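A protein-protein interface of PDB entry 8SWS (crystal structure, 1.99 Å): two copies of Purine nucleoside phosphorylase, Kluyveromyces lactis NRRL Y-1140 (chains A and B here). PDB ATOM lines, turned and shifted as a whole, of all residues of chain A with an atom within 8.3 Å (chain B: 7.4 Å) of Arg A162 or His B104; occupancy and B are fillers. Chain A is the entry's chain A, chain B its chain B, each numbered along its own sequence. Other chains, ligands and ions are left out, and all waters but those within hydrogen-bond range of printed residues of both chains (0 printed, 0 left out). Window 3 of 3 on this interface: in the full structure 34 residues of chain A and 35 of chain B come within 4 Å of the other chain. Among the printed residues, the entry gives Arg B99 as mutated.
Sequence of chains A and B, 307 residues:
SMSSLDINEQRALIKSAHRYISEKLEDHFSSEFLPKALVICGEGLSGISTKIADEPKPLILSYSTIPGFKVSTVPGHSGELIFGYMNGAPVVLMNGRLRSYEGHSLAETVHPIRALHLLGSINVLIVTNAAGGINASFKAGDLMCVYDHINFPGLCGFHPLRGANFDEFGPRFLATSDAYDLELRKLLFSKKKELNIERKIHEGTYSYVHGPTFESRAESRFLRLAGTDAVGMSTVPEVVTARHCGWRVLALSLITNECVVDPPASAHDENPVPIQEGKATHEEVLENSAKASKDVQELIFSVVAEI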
ATOM      1  N   ILE A   7      -6.475 -16.183  26.752  1.00  0.00           N
ATOM      2  CA  ILE A   7      -6.214 -17.464  26.105  1.00  0.00           C
ATOM      3  C   ILE A   7      -4.810 -17.968  26.425  1.00  0.00           C
ATOM      4  O   ILE A   7      -4.620 -19.169  26.639  1.00  0.00           O
ATOM      5  CB  ILE A   7      -6.495 -17.396  24.590  1.00  0.00           C
ATOM      6  CG1 ILE A   7      -6.674 -18.825  24.057  1.00  0.00           C
ATOM      7  CG2 ILE A   7      -5.424 -16.585  23.832  1.00  0.00           C
ATOM      8  CD1 ILE A   7      -7.385 -18.909  22.751  1.00  0.00           C
ATOM      9  N   GLN A  10      -4.772 -19.659  29.530  1.00  0.00           N
ATOM     10  CA  GLN A  10      -5.453 -20.919  29.346  1.00  0.00           C
ATOM     11  C   GLN A  10      -4.567 -21.921  28.620  1.00  0.00           C
ATOM     12  O   GLN A  10      -4.537 -23.097  28.995  1.00  0.00           O
ATOM     13  CB  GLN A  10      -6.759 -20.665  28.610  1.00  0.00           C
ATOM     14  CG  GLN A  10      -7.921 -20.536  29.561  1.00  0.00           C
ATOM     15  CD  GLN A  10      -9.238 -20.418  28.836  1.00  0.00           C
ATOM     16  OE1 GLN A  10      -9.669 -19.307  28.527  1.00  0.00           O
ATOM     17  NE2 GLN A  10      -9.892 -21.549  28.569  1.00  0.00           N
ATOM     18  N   LEU A 106     -17.607 -21.974  32.706  1.00  0.00           N
ATOM     19  CA  LEU A 106     -17.715 -23.075  31.756  1.00  0.00           C
ATOM     20  C   LEU A 106     -16.343 -23.488  31.249  1.00  0.00           C
ATOM     21  O   LEU A 106     -16.082 -24.682  31.056  1.00  0.00           O
ATOM     22  CB  LEU A 106     -18.631 -22.703  30.590  1.00  0.00           C
ATOM     23  CG  LEU A 106     -20.112 -22.660  30.952  1.00  0.00           C
ATOM     24  CD1 LEU A 106     -20.927 -22.059  29.791  1.00  0.00           C
ATOM     25  CD2 LEU A 106     -20.630 -24.047  31.326  1.00  0.00           C
ATOM     26  N   ALA A 107     -15.444 -22.520  31.057  1.00  0.00           N
ATOM     27  CA  ALA A 107     -14.082 -22.862  30.660  1.00  0.00           C
ATOM     28  C   ALA A 107     -13.431 -23.801  31.670  1.00  0.00           C
ATOM     29  O   ALA A 107     -12.694 -24.719  31.289  1.00  0.00           O
ATOM     30  CB  ALA A 107     -13.246 -21.595  30.478  1.00  0.00           C
ATOM     31  N   ARG A 114      -9.713 -30.376  27.018  1.00  0.00           N
ATOM     32  CA  ARG A 114      -8.569 -29.803  26.297  1.00  0.00           C
ATOM     33  C   ARG A 114      -7.252 -30.450  26.724  1.00  0.00           C
ATOM     34  O   ARG A 114      -6.413 -30.802  25.883  1.00  0.00           O
ATOM     35  CB  ARG A 114      -8.492 -28.285  26.527  1.00  0.00           C
ATOM     36  CG  ARG A 114      -9.803 -27.523  26.421  1.00  0.00           C
ATOM     37  CD  ARG A 114     -10.178 -27.366  24.982  1.00  0.00           C
ATOM     38  NE  ARG A 114     -11.017 -26.206  24.682  1.00  0.00           N
ATOM     39  CZ  ARG A 114     -11.426 -25.921  23.446  1.00  0.00           C
ATOM     40  NH1 ARG A 114     -11.122 -26.709  22.416  1.00  0.00           N
ATOM     41  NH2 ARG A 114     -12.203 -24.860  23.240  1.00  0.00           N
ATOM     42  N   GLY A 154     -26.176 -21.317  26.238  1.00  0.00           N
ATOM     43  CA  GLY A 154     -25.278 -20.899  25.156  1.00  0.00           C
ATOM     44  C   GLY A 154     -25.873 -19.845  24.237  1.00  0.00           C
ATOM     45  O   GLY A 154     -25.218 -18.837  23.924  1.00  0.00           O
ATOM     46  N   CYS A 156     -27.869 -17.653  24.991  1.00  0.00           N
ATOM     47  CA  CYS A 156     -28.069 -16.439  25.774  1.00  0.00           C
ATOM     48  C   CYS A 156     -26.768 -15.899  26.373  1.00  0.00           C
ATOM     49  O   CYS A 156     -26.813 -14.993  27.227  1.00  0.00           O
ATOM     50  CB  CYS A 156     -29.093 -16.713  26.890  1.00  0.00           C
ATOM     51  SG  CYS A 156     -30.774 -17.037  26.272  1.00  0.00           S
ATOM     52  N   GLY A 157     -25.612 -16.429  25.969  1.00  0.00           N
ATOM     53  CA  GLY A 157     -24.352 -15.852  26.368  1.00  0.00           C
ATOM     54  C   GLY A 157     -23.511 -16.665  27.325  1.00  0.00           C
ATOM     55  O   GLY A 157     -22.405 -16.216  27.646  1.00  0.00           O
ATOM     56  N   PHE A 158     -23.964 -17.840  27.795  1.00  0.00           N
ATOM     57  CA  PHE A 158     -23.135 -18.692  28.664  1.00  0.00           C
ATOM     58  C   PHE A 158     -22.645 -19.893  27.864  1.00  0.00           C
ATOM     59  O   PHE A 158     -23.305 -20.929  27.782  1.00  0.00           O
ATOM     60  CB  PHE A 158     -23.911 -19.123  29.928  1.00  0.00           C
ATOM     61  CG  PHE A 158     -24.244 -17.960  30.822  1.00  0.00           C
ATOM     62  CD1 PHE A 158     -23.464 -17.687  31.948  1.00  0.00           C
ATOM     63  CD2 PHE A 158     -25.351 -17.151  30.556  1.00  0.00           C
ATOM     64  CE1 PHE A 158     -23.754 -16.593  32.790  1.00  0.00           C
ATOM     65  CE2 PHE A 158     -25.650 -16.080  31.385  1.00  0.00           C
ATOM     66  CZ  PHE A 158     -24.850 -15.804  32.518  1.00  0.00           C
ATOM     67  N   HIS A 159     -21.465 -19.751  27.276  1.00  0.00           N
ATOM     68  CA  HIS A 159     -21.078 -20.672  26.211  1.00  0.00           C
ATOM     69  C   HIS A 159     -19.631 -21.086  26.438  1.00  0.00           C
ATOM     70  O   HIS A 159     -18.781 -20.222  26.682  1.00  0.00           O
ATOM     71  CB  HIS A 159     -21.245 -19.976  24.849  1.00  0.00           C
ATOM     72  CG  HIS A 159     -21.235 -20.921  23.690  1.00  0.00           C
ATOM     73  ND1 HIS A 159     -20.144 -21.718  23.398  1.00  0.00           N
ATOM     74  CD2 HIS A 159     -22.178 -21.208  22.762  1.00  0.00           C
ATOM     75  CE1 HIS A 159     -20.425 -22.472  22.339  1.00  0.00           C
ATOM     76  NE2 HIS A 159     -21.652 -22.180  21.937  1.00  0.00           N
ATOM     77  N   PRO A 160     -19.313 -22.377  26.368  1.00  0.00           N
ATOM     78  CA  PRO A 160     -17.928 -22.793  26.639  1.00  0.00           C
ATOM     79  C   PRO A 160     -16.917 -22.349  25.601  1.00  0.00           C
ATOM     80  O   PRO A 160     -15.716 -22.362  25.907  1.00  0.00           O
ATOM     81  CB  PRO A 160     -18.037 -24.323  26.706  1.00  0.00           C
ATOM     82  CG  PRO A 160     -19.204 -24.647  25.750  1.00  0.00           C
ATOM     83  CD  PRO A 160     -20.197 -23.520  26.052  1.00  0.00           C
ATOM     84  N   LEU A 161     -17.320 -21.966  24.386  1.00  0.00           N
ATOM     85  CA  LEU A 161     -16.356 -21.474  23.394  1.00  0.00           C
ATOM     86  C   LEU A 161     -16.227 -19.949  23.354  1.00  0.00           C
ATOM     87  O   LEU A 161     -15.435 -19.429  22.545  1.00  0.00           O
ATOM     88  CB  LEU A 161     -16.703 -21.995  21.996  1.00  0.00           C
ATOM     89  CG  LEU A 161     -16.906 -23.523  21.880  1.00  0.00           C
ATOM     90  CD1 LEU A 161     -17.297 -23.932  20.420  1.00  0.00           C
ATOM     91  CD2 LEU A 161     -15.634 -24.276  22.354  1.00  0.00           C
ATOM     92  N   ARG A 162     -16.971 -19.226  24.188  1.00  0.00           N
ATOM     93  CA  ARG A 162     -16.791 -17.773  24.291  1.00  0.00           C
ATOM     94  C   ARG A 162     -15.332 -17.406  24.552  1.00  0.00           C
ATOM     95  O   ARG A 162     -14.654 -18.027  25.373  1.00  0.00           O
ATOM     96  CB  ARG A 162     -17.659 -17.200  25.412  1.00  0.00           C
ATOM     97  CG  ARG A 162     -17.507 -15.673  25.623  1.00  0.00           C
ATOM     98  CD  ARG A 162     -18.686 -15.085  26.403  1.00  0.00           C
ATOM     99  NE  ARG A 162     -18.898 -13.675  26.070  1.00  0.00           N
ATOM    100  CZ  ARG A 162     -18.283 -12.717  26.744  1.00  0.00           C
ATOM    101  NH1 ARG A 162     -17.496 -13.006  27.769  1.00  0.00           N
ATOM    102  NH2 ARG A 162     -18.450 -11.441  26.385  1.00  0.00           N
ATOM    103  N   GLY A 163     -14.865 -16.362  23.870  1.00  0.00           N
ATOM    104  CA  GLY A 163     -13.498 -15.892  23.951  1.00  0.00           C
ATOM    105  C   GLY A 163     -12.747 -16.249  22.687  1.00  0.00           C
ATOM    106  O   GLY A 163     -13.280 -16.865  21.758  1.00  0.00           O
ATOM    107  N   ALA A 164     -11.467 -15.892  22.695  1.00  0.00           N
ATOM    108  CA  ALA A 164     -10.609 -16.237  21.571  1.00  0.00           C
ATOM    109  C   ALA A 164     -10.671 -17.739  21.304  1.00  0.00           C
ATOM    110  O   ALA A 164     -10.847 -18.558  22.226  1.00  0.00           O
ATOM    111  CB  ALA A 164      -9.165 -15.799  21.830  1.00  0.00           C
ATOM    112  N   ASN A 165     -10.567 -18.092  20.021  1.00  0.00           N
ATOM    113  CA  ASN A 165     -10.656 -19.487  19.604  1.00  0.00           C
ATOM    114  C   ASN A 165      -9.321 -20.187  19.789  1.00  0.00           C
ATOM    115  O   ASN A 165      -8.262 -19.635  19.464  1.00  0.00           O
ATOM    116  CB  ASN A 165     -11.075 -19.609  18.141  1.00  0.00           C
ATOM    117  CG  ASN A 165     -11.258 -21.062  17.721  1.00  0.00           C
ATOM    118  OD1 ASN A 165     -11.999 -21.779  18.365  1.00  0.00           O
ATOM    119  ND2 ASN A 165     -10.555 -21.509  16.666  1.00  0.00           N
ATOM    120  N   PHE A 166      -9.379 -21.428  20.291  1.00  0.00           N
ATOM    121  CA  PHE A 166      -8.205 -22.296  20.343  1.00  0.00           C
ATOM    122  C   PHE A 166      -7.989 -22.841  18.942  1.00  0.00           C
ATOM    123  O   PHE A 166      -8.380 -23.964  18.614  1.00  0.00           O
ATOM    124  CB  PHE A 166      -8.385 -23.426  21.365  1.00  0.00           C
ATOM    125  CG  PHE A 166      -8.371 -22.953  22.805  1.00  0.00           C
ATOM    126  CD1 PHE A 166      -9.536 -22.535  23.427  1.00  0.00           C
ATOM    127  CD2 PHE A 166      -7.163 -22.830  23.498  1.00  0.00           C
ATOM    128  CE1 PHE A 166      -9.513 -22.056  24.748  1.00  0.00           C
ATOM    129  CE2 PHE A 166      -7.128 -22.348  24.813  1.00  0.00           C
ATOM    130  CZ  PHE A 166      -8.311 -21.968  25.437  1.00  0.00           C
ATOM    131  N   ARG A 172     -13.121 -21.770  14.592  1.00  0.00           N
ATOM    132  CA  ARG A 172     -13.833 -20.658  15.222  1.00  0.00           C
ATOM    133  C   ARG A 172     -15.339 -20.896  15.288  1.00  0.00           C
ATOM    134  O   ARG A 172     -15.987 -20.546  16.283  1.00  0.00           O
ATOM    135  CB  ARG A 172     -13.553 -19.360  14.447  1.00  0.00           C
ATOM    136  CG  ARG A 172     -14.334 -18.186  14.947  1.00  0.00           C
ATOM    137  CD  ARG A 172     -13.975 -17.534  16.337  1.00  0.00           C
ATOM    138  NE  ARG A 172     -14.570 -18.189  17.502  1.00  0.00           N
ATOM    139  CZ  ARG A 172     -14.292 -17.838  18.763  1.00  0.00           C
ATOM    140  NH1 ARG A 172     -13.611 -16.730  19.042  1.00  0.00           N
ATOM    141  NH2 ARG A 172     -14.755 -18.584  19.771  1.00  0.00           N
ATOM    142  N   VAL A 240     -19.891 -29.966  23.410  1.00  0.00           N
ATOM    143  CA  VAL A 240     -19.484 -28.907  22.494  1.00  0.00           C
ATOM    144  C   VAL A 240     -17.965 -28.848  22.412  1.00  0.00           C
ATOM    145  O   VAL A 240     -17.376 -28.801  21.315  1.00  0.00           O
ATOM    146  CB  VAL A 240     -20.094 -27.554  22.938  1.00  0.00           C
ATOM    147  CG1 VAL A 240     -19.447 -26.347  22.190  1.00  0.00           C
ATOM    148  CG2 VAL A 240     -21.600 -27.561  22.703  1.00  0.00           C
ATOM    149  N   LYS B  70     -11.000  -1.876  20.449  1.00  0.00           N
ATOM    150  CA  LYS B  70     -10.208  -3.005  20.941  1.00  0.00           C
ATOM    151  C   LYS B  70      -9.339  -3.646  19.853  1.00  0.00           C
ATOM    152  O   LYS B  70      -9.712  -3.682  18.684  1.00  0.00           O
ATOM    153  CB  LYS B  70     -11.132  -4.053  21.561  1.00  0.00           C
ATOM    154  CG  LYS B  70     -11.917  -3.512  22.742  1.00  0.00           C
ATOM    155  CD  LYS B  70     -11.039  -3.255  23.969  1.00  0.00           C
ATOM    156  CE  LYS B  70     -11.551  -2.029  24.758  1.00  0.00           C
ATOM    157  NZ  LYS B  70     -11.031  -1.917  26.155  1.00  0.00           N
ATOM    158  N   ARG B  97     -16.271  -5.475  12.609  1.00  0.00           N
ATOM    159  CA  ARG B  97     -17.219  -5.389  13.699  1.00  0.00           C
ATOM    160  C   ARG B  97     -16.716  -6.308  14.804  1.00  0.00           C
ATOM    161  O   ARG B  97     -15.897  -7.205  14.570  1.00  0.00           O
ATOM    162  CB  ARG B  97     -18.619  -5.795  13.196  1.00  0.00           C
ATOM    163  CG  ARG B  97     -18.965  -7.189  13.620  1.00  0.00           C
ATOM    164  CD  ARG B  97     -20.310  -7.621  13.193  1.00  0.00           C
ATOM    165  NE  ARG B  97     -21.414  -6.675  13.317  1.00  0.00           N
ATOM    166  CZ  ARG B  97     -22.339  -6.579  12.373  1.00  0.00           C
ATOM    167  NH1 ARG B  97     -22.261  -7.302  11.258  1.00  0.00           N
ATOM    168  NH2 ARG B  97     -23.351  -5.736  12.535  1.00  0.00           N
ATOM    169  N   LEU B  98     -17.192  -6.072  16.020  1.00  0.00           N
ATOM    170  CA  LEU B  98     -16.782  -6.837  17.188  1.00  0.00           C
ATOM    171  C   LEU B  98     -17.995  -7.606  17.690  1.00  0.00           C
ATOM    172  O   LEU B  98     -19.116  -7.090  17.666  1.00  0.00           O
ATOM    173  CB  LEU B  98     -16.227  -5.909  18.283  1.00  0.00           C
ATOM    174  CG  LEU B  98     -15.388  -4.769  17.687  1.00  0.00           C
ATOM    175  CD1 LEU B  98     -15.350  -3.525  18.582  1.00  0.00           C
ATOM    176  CD2 LEU B  98     -13.983  -5.247  17.342  1.00  0.00           C
ATOM    177  N   ARG B  99     -17.778  -8.837  18.131  1.00  0.00           N
ATOM    178  CA  ARG B  99     -18.873  -9.731  18.461  1.00  0.00           C
ATOM    179  C   ARG B  99     -18.633 -10.266  19.849  1.00  0.00           C
ATOM    180  O   ARG B  99     -17.488 -10.502  20.236  1.00  0.00           O
ATOM    181  CB  ARG B  99     -18.890 -10.857  17.465  1.00  0.00           C
ATOM    182  CG  ARG B  99     -19.559 -10.401  16.224  1.00  0.00           C
ATOM    183  CD  ARG B  99     -18.881 -11.147  15.179  1.00  0.00           C
ATOM    184  NE  ARG B  99     -19.153 -10.699  13.833  1.00  0.00           N
ATOM    185  CZ  ARG B  99     -18.176 -10.426  12.988  1.00  0.00           C
ATOM    186  NH1 ARG B  99     -16.912 -10.355  13.400  1.00  0.00           N
ATOM    187  NH2 ARG B  99     -18.474 -10.162  11.716  1.00  0.00           N
ATOM    188  N   SER B 100     -19.720 -10.446  20.591  1.00  0.00           N
ATOM    189  CA  SER B 100     -19.582 -10.867  21.975  1.00  0.00           C
ATOM    190  C   SER B 100     -18.946 -12.250  22.084  1.00  0.00           C
ATOM    191  O   SER B 100     -18.216 -12.505  23.045  1.00  0.00           O
ATOM    192  CB  SER B 100     -20.938 -10.833  22.687  1.00  0.00           C
ATOM    193  OG  SER B 100     -20.808 -11.307  24.042  1.00  0.00           O
ATOM    194  N   TYR B 101     -19.151 -13.144  21.096  1.00  0.00           N
ATOM    195  CA  TYR B 101     -18.511 -14.451  21.244  1.00  0.00           C
ATOM    196  C   TYR B 101     -16.989 -14.352  21.227  1.00  0.00           C
ATOM    197  O   TYR B 101     -16.321 -15.307  21.657  1.00  0.00           O
ATOM    198  CB  TYR B 101     -18.969 -15.429  20.160  1.00  0.00           C
ATOM    199  CG  TYR B 101     -18.645 -15.007  18.737  1.00  0.00           C
ATOM    200  CD1 TYR B 101     -17.330 -15.044  18.254  1.00  0.00           C
ATOM    201  CD2 TYR B 101     -19.642 -14.597  17.884  1.00  0.00           C
ATOM    202  CE1 TYR B 101     -17.027 -14.698  16.957  1.00  0.00           C
ATOM    203  CE2 TYR B 101     -19.349 -14.241  16.550  1.00  0.00           C
ATOM    204  CZ  TYR B 101     -18.023 -14.295  16.105  1.00  0.00           C
ATOM    205  OH  TYR B 101     -17.681 -13.934  14.819  1.00  0.00           O
ATOM    206  N   GLU B 102     -16.432 -13.235  20.720  1.00  0.00           N
ATOM    207  CA  GLU B 102     -14.982 -13.033  20.721  1.00  0.00           C
ATOM    208  C   GLU B 102     -14.447 -12.817  22.139  1.00  0.00           C
ATOM    209  O   GLU B 102     -13.228 -12.834  22.357  1.00  0.00           O
ATOM    210  CB  GLU B 102     -14.592 -11.842  19.815  1.00  0.00           C
ATOM    211  CG  GLU B 102     -14.866 -12.069  18.321  1.00  0.00           C
ATOM    212  CD  GLU B 102     -15.214 -10.802  17.457  1.00  0.00           C
ATOM    213  OE1 GLU B 102     -14.958 -10.825  16.219  1.00  0.00           O
ATOM    214  OE2 GLU B 102     -15.660  -9.756  17.980  1.00  0.00           O
ATOM    215  N   GLY B 103     -15.327 -12.654  23.122  1.00  0.00           N
ATOM    216  CA  GLY B 103     -14.922 -12.355  24.476  1.00  0.00           C
ATOM    217  C   GLY B 103     -14.963 -10.879  24.818  1.00  0.00           C
ATOM    218  O   GLY B 103     -14.557 -10.504  25.921  1.00  0.00           O
ATOM    219  N   HIS B 104     -15.439 -10.037  23.909  1.00  0.00           N
ATOM    220  CA  HIS B 104     -15.576  -8.609  24.183  1.00  0.00           C
ATOM    221  C   HIS B 104     -16.872  -8.347  24.937  1.00  0.00           C
ATOM    222  O   HIS B 104     -17.884  -9.013  24.696  1.00  0.00           O
ATOM    223  CB  HIS B 104     -15.560  -7.838  22.864  1.00  0.00           C
ATOM    224  CG  HIS B 104     -14.254  -7.945  22.135  1.00  0.00           C
ATOM    225  ND1 HIS B 104     -14.169  -8.262  20.794  1.00  0.00           N
ATOM    226  CD2 HIS B 104     -12.979  -7.789  22.567  1.00  0.00           C
ATOM    227  CE1 HIS B 104     -12.898  -8.304  20.434  1.00  0.00           C
ATOM    228  NE2 HIS B 104     -12.155  -8.008  21.488  1.00  0.00           N
ATOM    229  N   SER B 105     -16.836  -7.389  25.867  1.00  0.00           N
ATOM    230  CA  SER B 105     -18.082  -6.922  26.464  1.00  0.00           C
ATOM    231  C   SER B 105     -18.929  -6.210  25.411  1.00  0.00           C
ATOM    232  O   SER B 105     -18.421  -5.705  24.397  1.00  0.00           O
ATOM    233  CB  SER B 105     -17.824  -5.959  27.612  1.00  0.00           C
ATOM    234  OG  SER B 105     -17.205  -4.785  27.117  1.00  0.00           O
ATOM    235  N   LEU B 106     -20.239  -6.163  25.665  1.00  0.00           N
ATOM    236  CA  LEU B 106     -21.120  -5.498  24.712  1.00  0.00           C
ATOM    237  C   LEU B 106     -20.823  -4.007  24.646  1.00  0.00           C
ATOM    238  O   LEU B 106     -20.960  -3.395  23.575  1.00  0.00           O
ATOM    239  CB  LEU B 106     -22.584  -5.751  25.076  1.00  0.00           C
ATOM    240  CG  LEU B 106     -23.083  -7.152  24.700  1.00  0.00           C
ATOM    241  CD1 LEU B 106     -24.612  -7.219  24.718  1.00  0.00           C
ATOM    242  CD2 LEU B 106     -22.536  -7.585  23.318  1.00  0.00           C
ATOM    243  N   ALA B 107     -20.396  -3.415  25.766  1.00  0.00           N
ATOM    244  CA  ALA B 107     -19.961  -2.022  25.748  1.00  0.00           C
ATOM    245  C   ALA B 107     -18.796  -1.832  24.784  1.00  0.00           C
ATOM    246  O   ALA B 107     -18.764  -0.860  24.012  1.00  0.00           O
ATOM    247  CB  ALA B 107     -19.569  -1.561  27.153  1.00  0.00           C
ATOM    248  N   GLU B 108     -17.840  -2.763  24.796  1.00  0.00           N
ATOM    249  CA  GLU B 108     -16.702  -2.616  23.901  1.00  0.00           C
ATOM    250  C   GLU B 108     -17.161  -2.727  22.462  1.00  0.00           C
ATOM    251  O   GLU B 108     -16.619  -2.057  21.577  1.00  0.00           O
ATOM    252  CB  GLU B 108     -15.650  -3.681  24.177  1.00  0.00           C
ATOM    253  CG  GLU B 108     -14.629  -3.232  25.207  1.00  0.00           C
ATOM    254  CD  GLU B 108     -14.150  -4.398  26.043  1.00  0.00           C
ATOM    255  OE1 GLU B 108     -12.924  -4.517  26.269  1.00  0.00           O
ATOM    256  OE2 GLU B 108     -14.970  -5.308  26.306  1.00  0.00           O
ATOM    257  N   THR B 109     -18.188  -3.553  22.225  1.00  0.00           N
ATOM    258  CA  THR B 109     -18.726  -3.799  20.894  1.00  0.00           C
ATOM    259  C   THR B 109     -19.366  -2.549  20.298  1.00  0.00           C
ATOM    260  O   THR B 109     -19.311  -2.344  19.075  1.00  0.00           O
ATOM    261  CB  THR B 109     -19.735  -4.951  21.002  1.00  0.00           C
ATOM    262  OG1 THR B 109     -19.024  -6.185  21.233  1.00  0.00           O
ATOM    263  CG2 THR B 109     -20.603  -5.033  19.804  1.00  0.00           C
ATOM    264  N   PHE B 158     -27.194  -9.249  29.512  1.00  0.00           N
ATOM    265  CA  PHE B 158     -26.068  -8.763  28.723  1.00  0.00           C
ATOM    266  C   PHE B 158     -26.601  -7.658  27.819  1.00  0.00           C
ATOM    267  O   PHE B 158     -27.336  -7.931  26.865  1.00  0.00           O
ATOM    268  CB  PHE B 158     -25.409  -9.888  27.925  1.00  0.00           C
ATOM    269  CG  PHE B 158     -24.962 -11.049  28.775  1.00  0.00           C
ATOM    270  CD1 PHE B 158     -23.830 -10.941  29.571  1.00  0.00           C
ATOM    271  CD2 PHE B 158     -25.632 -12.286  28.708  1.00  0.00           C
ATOM    272  CE1 PHE B 158     -23.413 -12.017  30.367  1.00  0.00           C
ATOM    273  CE2 PHE B 158     -25.212 -13.362  29.467  1.00  0.00           C
ATOM    274  CZ  PHE B 158     -24.097 -13.234  30.314  1.00  0.00           C
ATOM    275  N   HIS B 210     -25.832 -15.785  20.955  1.00  0.00           N
ATOM    276  CA  HIS B 210     -24.446 -15.485  21.288  1.00  0.00           C
ATOM    277  C   HIS B 210     -23.431 -16.148  20.355  1.00  0.00           C
ATOM    278  O   HIS B 210     -22.401 -15.543  20.025  1.00  0.00           O
ATOM    279  CB  HIS B 210     -24.183 -15.893  22.727  1.00  0.00           C
ATOM    280  CG  HIS B 210     -22.827 -15.506  23.217  1.00  0.00           C
ATOM    281  ND1 HIS B 210     -21.744 -16.360  23.126  1.00  0.00           N
ATOM    282  CD2 HIS B 210     -22.367 -14.366  23.784  1.00  0.00           C
ATOM    283  CE1 HIS B 210     -20.679 -15.761  23.640  1.00  0.00           C
ATOM    284  NE2 HIS B 210     -21.032 -14.557  24.051  1.00  0.00           N
ATOM    285  N   GLY B 211     -23.633 -17.418  19.993  1.00  0.00           N
ATOM    286  CA  GLY B 211     -22.607 -18.117  19.226  1.00  0.00           C
ATOM    287  C   GLY B 211     -21.478 -18.591  20.131  1.00  0.00           C
ATOM    288  O   GLY B 211     -21.578 -18.515  21.360  1.00  0.00           O
ATOM    289  N   PRO B 212     -20.341 -19.047  19.557  1.00  0.00           N
ATOM    290  CA  PRO B 212     -19.977 -19.097  18.141  1.00  0.00           C
ATOM    291  C   PRO B 212     -20.420 -20.427  17.479  1.00  0.00           C
ATOM    292  O   PRO B 212     -19.960 -20.642  16.360  1.00  0.00           O
ATOM    293  CB  PRO B 212     -18.451 -19.015  18.179  1.00  0.00           C
ATOM    294  CG  PRO B 212     -18.108 -19.727  19.420  1.00  0.00           C
ATOM    295  CD  PRO B 212     -19.231 -19.504  20.406  1.00  0.00           C
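The guanidinium group (NE) of Arg A162 lies within hydrogen-bond range of a ring nitrogen (NE2) of His B210 (3.1 Å). O of Tyr B101 lies within hydrogen-bond range of N of Gly A163. O of His B104 sits at hydrogen-bond distance from NH2 of Arg A162. The guanidinium group (NE) of Arg A162 sits at hydrogen-bond distance from the backbone carbonyl oxygen (O) of Ser B100 (3.3 Å).
The backbone NH (N) of Leu A161 lies within hydrogen-bond range of a ring nitrogen (ND1) of His A159. O of Leu A161 sits at hydrogen-bond distance from NH2 of Arg A172 (3.0 Å). N of Arg A172 lies close to ND2 of Asn A165, 3.3 Å away. OG of Ser B100 lies within hydrogen-bond range of NE2 of His B210. OE1 of Glu B102 is in salt-bridge range of NH1 of Arg B99 (3.5 Å). The guanidinium group of Arg A172 sits at hydrogen-bond distance from the backbone carbonyl oxygen of Gly A163, at 2.7 Å.
His B210 touches Gly A157 (CG to CA, 3.5 Å). Phe A158 touches Phe B158. Gly B211 touches His A159 (O to CD2, 3.1 Å). Leu A161 touches Pro B212. Arg A162 touches Tyr B101. NH2 of Arg A162 touches C of Gly B103, at 3.9 Å. Gly A163 touches Glu B102 (CA to O, 3.5 Å). Gly A163 touches Gly B103. Ala A164 touches Glu B102 (N to O, 3.5 Å). Arg A172 touches Pro B212 (O to CB, 3.5 Å).
Of the printed residues of chain B, Gly A157 touches His B210 (3.5 Å). Printed residues of chain B within 4 Å of Leu A161: Pro B212 (3.7 Å). Arg A162 touches just these residues of chain B: Ser B100, Tyr B101, Gly B103, His B104 and His B210. Of the printed residues of chain A, Ser B100 touches Arg A162. Gly B103 touches just these residues of chain A: Arg A162 (3.9 Å) and Gly A163 (3.8 Å). Of the printed residues of chain A, His B104 touches Arg A162 (3.0 Å). No residue of chain A comes within 4 Å of Ser B105. Ala B107 touches none of the printed residues of chain A. Glu B108 touches none of the printed residues of chain A. Of the printed residues of chain A, Gly B211 touches His A159 (3.1 Å). The nearest printed residue of chain B that does not touch Arg A162 is Ser B105 (4.4 Å). The nearest residue of chain A that does not touch His B104 is Gly A163 (6.2 Å).
Of the 19 printed residues of chain A, 10 touch a printed residue of chain B. Among the printed residues, 17 pairs touch across the chains.
Phe B158 touches its own counterpart, Phe A158. Of the 17 pairs that touch across the chains among the printed residues, 1 has its exchanged pair printed and touching as well.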
